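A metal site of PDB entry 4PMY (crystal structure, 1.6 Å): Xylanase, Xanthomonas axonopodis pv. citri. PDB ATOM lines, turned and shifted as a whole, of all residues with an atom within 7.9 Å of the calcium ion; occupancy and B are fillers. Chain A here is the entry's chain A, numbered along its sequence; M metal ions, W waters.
The side-chain carboxylate (OE2) of Glu 93 lies within salt-bridge range of the guanidinium group (NH2) of Arg 45, at 2.8 Å. The indole nitrogen (NE1) of Trp 38 lies within hydrogen-bond range of the side-chain carboxylate (OE1) of Glu 42, 2.9 Å away. The backbone carbonyl oxygen of Glu 42 lies within hydrogen-bond range of the indole nitrogen of Trp 81.
Of the 15 residues printed, 4 come within 4 Å of the calcium ion. The nearest printed residue that does not touch the calcium ion is Trp 81 (4.7 Å).
The calcium ion is bound by the side-chain amide oxygen of Gln 96 (2.4 Å), water W2 (2.4 Å), the side-chain carboxylate of Asp 46 (2.4 Å), the side-chain carboxylate of Glu 42 (2.5 Å), water W1 (2.5 Å) and the side-chain carboxylate of Glu 93 (2.6 Å). The calcium ion has six donor atoms within binding distance.
Water W2 lies within hydrogen-bond range of the backbone carbonyl oxygen (O) of Glu 93, the side-chain carboxylate (OE1) of Glu 42 and the backbone NH (N) of Trp 97.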
ATOM      1  N   TRP A  38      14.316  26.351  19.142  1.00  0.00           N
ATOM      2  CA  TRP A  38      14.272  25.876  20.527  1.00  0.00           C
ATOM      3  C   TRP A  38      12.848  25.529  20.988  1.00  0.00           C
ATOM      4  O   TRP A  38      12.641  24.489  21.629  1.00  0.00           O
ATOM      5  CB  TRP A  38      14.928  26.896  21.454  1.00  0.00           C
ATOM      6  CG  TRP A  38      15.262  26.407  22.828  1.00  0.00           C
ATOM      7  CD1 TRP A  38      15.102  25.136  23.335  1.00  0.00           C
ATOM      8  CD2 TRP A  38      15.861  27.179  23.869  1.00  0.00           C
ATOM      9  NE1 TRP A  38      15.546  25.087  24.627  1.00  0.00           N
ATOM     10  CE2 TRP A  38      16.018  26.322  24.987  1.00  0.00           C
ATOM     11  CE3 TRP A  38      16.282  28.513  23.967  1.00  0.00           C
ATOM     12  CZ2 TRP A  38      16.583  26.761  26.191  1.00  0.00           C
ATOM     13  CZ3 TRP A  38      16.826  28.947  25.176  1.00  0.00           C
ATOM     14  CH2 TRP A  38      16.974  28.077  26.260  1.00  0.00           C
ATOM     15  N   GLU A  42      11.944  21.973  22.517  1.00  0.00           N
ATOM     16  CA  GLU A  42      11.669  21.948  23.944  1.00  0.00           C
ATOM     17  C   GLU A  42      10.448  22.797  24.300  1.00  0.00           C
ATOM     18  O   GLU A  42      10.523  23.685  25.153  1.00  0.00           O
ATOM     19  CB  GLU A  42      12.903  22.400  24.733  1.00  0.00           C
ATOM     20  CG  GLU A  42      12.898  21.952  26.195  1.00  0.00           C
ATOM     21  CD  GLU A  42      14.210  22.245  26.903  1.00  0.00           C
ATOM     22  OE1 GLU A  42      15.172  22.715  26.267  1.00  0.00           O
ATOM     23  OE2 GLU A  42      14.276  22.000  28.135  1.00  0.00           O
ATOM     24  N   VAL A  44       7.885  21.694  25.833  1.00  0.00           N
ATOM     25  CA  VAL A  44       7.675  21.337  27.230  1.00  0.00           C
ATOM     26  C   VAL A  44       9.048  21.188  27.873  1.00  0.00           C
ATOM     27  O   VAL A  44       9.904  20.458  27.376  1.00  0.00           O
ATOM     28  CB  VAL A  44       6.851  20.044  27.357  1.00  0.00           C
ATOM     29  CG1 VAL A  44       6.695  19.641  28.824  1.00  0.00           C
ATOM     30  CG2 VAL A  44       5.476  20.218  26.713  1.00  0.00           C
ATOM     31  N   ARG A  45       9.258  21.911  28.972  1.00  0.00           N
ATOM     32  CA  ARG A  45      10.561  22.007  29.612  1.00  0.00           C
ATOM     33  C   ARG A  45      11.176  20.645  29.944  1.00  0.00           C
ATOM     34  O   ARG A  45      10.515  19.782  30.508  1.00  0.00           O
ATOM     35  CB  ARG A  45      10.477  22.879  30.865  1.00  0.00           C
ATOM     36  CG  ARG A  45      11.835  23.285  31.409  1.00  0.00           C
ATOM     37  CD  ARG A  45      11.709  23.897  32.788  1.00  0.00           C
ATOM     38  NE  ARG A  45      12.972  24.490  33.214  1.00  0.00           N
ATOM     39  CZ  ARG A  45      13.109  25.279  34.284  1.00  0.00           C
ATOM     40  NH1 ARG A  45      12.050  25.560  35.040  1.00  0.00           N
ATOM     41  NH2 ARG A  45      14.295  25.786  34.583  1.00  0.00           N
ATOM     42  N   ASP A  46      12.445  20.485  29.564  1.00  0.00           N
ATOM     43  CA  ASP A  46      13.262  19.293  29.827  1.00  0.00           C
ATOM     44  C   ASP A  46      12.758  17.987  29.199  1.00  0.00           C
ATOM     45  O   ASP A  46      13.220  16.907  29.556  1.00  0.00           O
ATOM     46  CB  ASP A  46      13.548  19.129  31.326  1.00  0.00           C
ATOM     47  CG  ASP A  46      14.270  20.336  31.922  1.00  0.00           C
ATOM     48  OD1 ASP A  46      15.010  21.032  31.186  1.00  0.00           O
ATOM     49  OD2 ASP A  46      14.091  20.594  33.130  1.00  0.00           O
ATOM     50  N   GLN A  47      11.831  18.089  28.257  1.00  0.00           N
ATOM     51  CA  GLN A  47      11.597  16.989  27.323  1.00  0.00           C
ATOM     52  C   GLN A  47      11.876  17.427  25.896  1.00  0.00           C
ATOM     53  O   GLN A  47      11.272  18.381  25.388  1.00  0.00           O
ATOM     54  CB  GLN A  47      10.242  16.294  27.512  1.00  0.00           C
ATOM     55  CG  GLN A  47       8.999  17.101  27.173  1.00  0.00           C
ATOM     56  CD  GLN A  47       7.728  16.414  27.636  1.00  0.00           C
ATOM     57  OE1 GLN A  47       7.651  15.913  28.767  1.00  0.00           O
ATOM     58  NE2 GLN A  47       6.714  16.386  26.775  1.00  0.00           N
ATOM     59  N   MET A  48      12.834  16.772  25.280  1.00  0.00           N
ATOM     60  CA  MET A  48      13.339  17.206  23.983  1.00  0.00           C
ATOM     61  C   MET A  48      12.670  16.394  22.881  1.00  0.00           C
ATOM     62  O   MET A  48      12.797  15.178  22.837  1.00  0.00           O
ATOM     63  CB  MET A  48      14.861  17.063  23.927  1.00  0.00           C
ATOM     64  CG  MET A  48      15.613  17.688  25.094  1.00  0.00           C
ATOM     65  SD  MET A  48      15.462  19.479  25.194  1.00  0.00           S
ATOM     66  CE  MET A  48      16.776  20.015  24.103  1.00  0.00           C
ATOM     67  N   TRP A  81       7.889  28.450  28.365  1.00  0.00           N
ATOM     68  CA  TRP A  81       8.205  28.390  29.795  1.00  0.00           C
ATOM     69  C   TRP A  81       9.425  29.234  30.191  1.00  0.00           C
ATOM     70  O   TRP A  81       9.573  29.582  31.365  1.00  0.00           O
ATOM     71  CB  TRP A  81       8.391  26.937  30.259  1.00  0.00           C
ATOM     72  CG  TRP A  81       9.329  26.162  29.390  1.00  0.00           C
ATOM     73  CD1 TRP A  81       8.991  25.347  28.359  1.00  0.00           C
ATOM     74  CD2 TRP A  81      10.768  26.175  29.450  1.00  0.00           C
ATOM     75  NE1 TRP A  81      10.124  24.828  27.772  1.00  0.00           N
ATOM     76  CE2 TRP A  81      11.228  25.327  28.419  1.00  0.00           C
ATOM     77  CE3 TRP A  81      11.702  26.813  30.277  1.00  0.00           C
ATOM     78  CZ2 TRP A  81      12.592  25.098  28.187  1.00  0.00           C
ATOM     79  CZ3 TRP A  81      13.054  26.583  30.051  1.00  0.00           C
ATOM     80  CH2 TRP A  81      13.482  25.738  29.004  1.00  0.00           C
ATOM     81  N   ARG A  92      21.279  28.984  32.367  1.00  0.00           N
ATOM     82  CA  ARG A  92      21.562  27.563  32.514  1.00  0.00           C
ATOM     83  C   ARG A  92      20.792  26.742  31.478  1.00  0.00           C
ATOM     84  O   ARG A  92      21.323  25.783  30.914  1.00  0.00           O
ATOM     85  CB  ARG A  92      21.267  27.092  33.937  1.00  0.00           C
ATOM     86  CG  ARG A  92      22.132  27.804  34.961  1.00  0.00           C
ATOM     87  CD  ARG A  92      21.734  27.401  36.377  1.00  0.00           C
ATOM     88  NE  ARG A  92      22.105  26.022  36.652  1.00  0.00           N
ATOM     89  CZ  ARG A  92      21.456  25.205  37.475  1.00  0.00           C
ATOM     90  NH1 ARG A  92      20.378  25.612  38.128  1.00  0.00           N
ATOM     91  NH2 ARG A  92      21.900  23.973  37.645  1.00  0.00           N
ATOM     92  N   GLU A  93      19.546  27.148  31.216  1.00  0.00           N
ATOM     93  CA  GLU A  93      18.734  26.553  30.150  1.00  0.00           C
ATOM     94  C   GLU A  93      19.353  26.755  28.775  1.00  0.00           C
ATOM     95  O   GLU A  93      19.380  25.832  27.962  1.00  0.00           O
ATOM     96  CB  GLU A  93      17.305  27.101  30.180  1.00  0.00           C
ATOM     97  CG  GLU A  93      16.473  26.671  31.384  1.00  0.00           C
ATOM     98  CD  GLU A  93      16.112  25.189  31.370  1.00  0.00           C
ATOM     99  OE1 GLU A  93      16.326  24.496  30.357  1.00  0.00           O
ATOM    100  OE2 GLU A  93      15.622  24.699  32.413  1.00  0.00           O
ATOM    101  N   ILE A  94      19.850  27.962  28.513  1.00  0.00           N
ATOM    102  CA  ILE A  94      20.512  28.264  27.231  1.00  0.00           C
ATOM    103  C   ILE A  94      21.758  27.392  27.076  1.00  0.00           C
ATOM    104  O   ILE A  94      21.957  26.767  26.024  1.00  0.00           O
ATOM    105  CB  ILE A  94      20.866  29.758  27.092  1.00  0.00           C
ATOM    106  CG1 ILE A  94      19.598  30.625  27.096  1.00  0.00           C
ATOM    107  CG2 ILE A  94      21.670  30.006  25.816  1.00  0.00           C
ATOM    108  CD1 ILE A  94      19.854  32.097  27.352  1.00  0.00           C
ATOM    109  N   GLU A  95      22.578  27.341  28.124  1.00  0.00           N
ATOM    110  CA  GLU A  95      23.769  26.483  28.140  1.00  0.00           C
ATOM    111  C   GLU A  95      23.430  25.022  27.816  1.00  0.00           C
ATOM    112  O   GLU A  95      24.076  24.400  26.969  1.00  0.00           O
ATOM    113  CB  GLU A  95      24.467  26.577  29.506  1.00  0.00           C
ATOM    114  CG  GLU A  95      25.180  27.890  29.786  1.00  0.00           C
ATOM    115  CD  GLU A  95      26.694  27.796  29.654  1.00  0.00           C
ATOM    116  OE1 GLU A  95      27.375  28.698  30.170  1.00  0.00           O
ATOM    117  OE2 GLU A  95      27.199  26.819  29.039  1.00  0.00           O
ATOM    118  N   GLN A  96      22.387  24.499  28.475  1.00  0.00           N
ATOM    119  CA  GLN A  96      21.951  23.115  28.250  1.00  0.00           C
ATOM    120  C   GLN A  96      21.481  22.877  26.817  1.00  0.00           C
ATOM    121  O   GLN A  96      21.802  21.846  26.226  1.00  0.00           O
ATOM    122  CB  GLN A  96      20.861  22.716  29.248  1.00  0.00           C
ATOM    123  CG  GLN A  96      20.347  21.300  29.038  1.00  0.00           C
ATOM    124  CD  GLN A  96      19.488  20.795  30.181  1.00  0.00           C
ATOM    125  OE1 GLN A  96      18.399  21.303  30.434  1.00  0.00           O
ATOM    126  NE2 GLN A  96      19.973  19.762  30.850  1.00  0.00           N
ATOM    127  N   TRP A  97      20.730  23.839  26.273  1.00  0.00           N
ATOM    128  CA  TRP A  97      20.265  23.793  24.884  1.00  0.00           C
ATOM    129  C   TRP A  97      21.426  23.704  23.882  1.00  0.00           C
ATOM    130  O   TRP A  97      21.401  22.881  22.963  1.00  0.00           O
ATOM    131  CB  TRP A  97      19.360  25.013  24.639  1.00  0.00           C
ATOM    132  CG  TRP A  97      19.035  25.420  23.211  1.00  0.00           C
ATOM    133  CD1 TRP A  97      19.246  26.657  22.660  1.00  0.00           C
ATOM    134  CD2 TRP A  97      18.420  24.627  22.185  1.00  0.00           C
ATOM    135  NE1 TRP A  97      18.807  26.678  21.360  1.00  0.00           N
ATOM    136  CE2 TRP A  97      18.298  25.454  21.038  1.00  0.00           C
ATOM    137  CE3 TRP A  97      17.952  23.307  22.118  1.00  0.00           C
ATOM    138  CZ2 TRP A  97      17.734  24.990  19.834  1.00  0.00           C
ATOM    139  CZ3 TRP A  97      17.393  22.856  20.911  1.00  0.00           C
ATOM    140  CH2 TRP A  97      17.292  23.696  19.791  1.00  0.00           C
ATOM    141  N   ALA A 100      23.083  20.311  24.339  1.00  0.00           N
ATOM    142  CA  ALA A 100      22.195  19.256  23.824  1.00  0.00           C
ATOM    143  C   ALA A 100      22.330  19.118  22.324  1.00  0.00           C
ATOM    144  O   ALA A 100      22.460  18.008  21.801  1.00  0.00           O
ATOM    145  CB  ALA A 100      20.759  19.534  24.215  1.00  0.00           C
HETATM  146 CA    CA M   1      16.365  22.105  29.469  1.00  0.00          CA
HETATM  147  O   HOH W   1      16.894  20.005  28.216  1.00  0.00           O
HETATM  148  O   HOH W   2      17.697  23.448  27.950  1.00  0.00           O
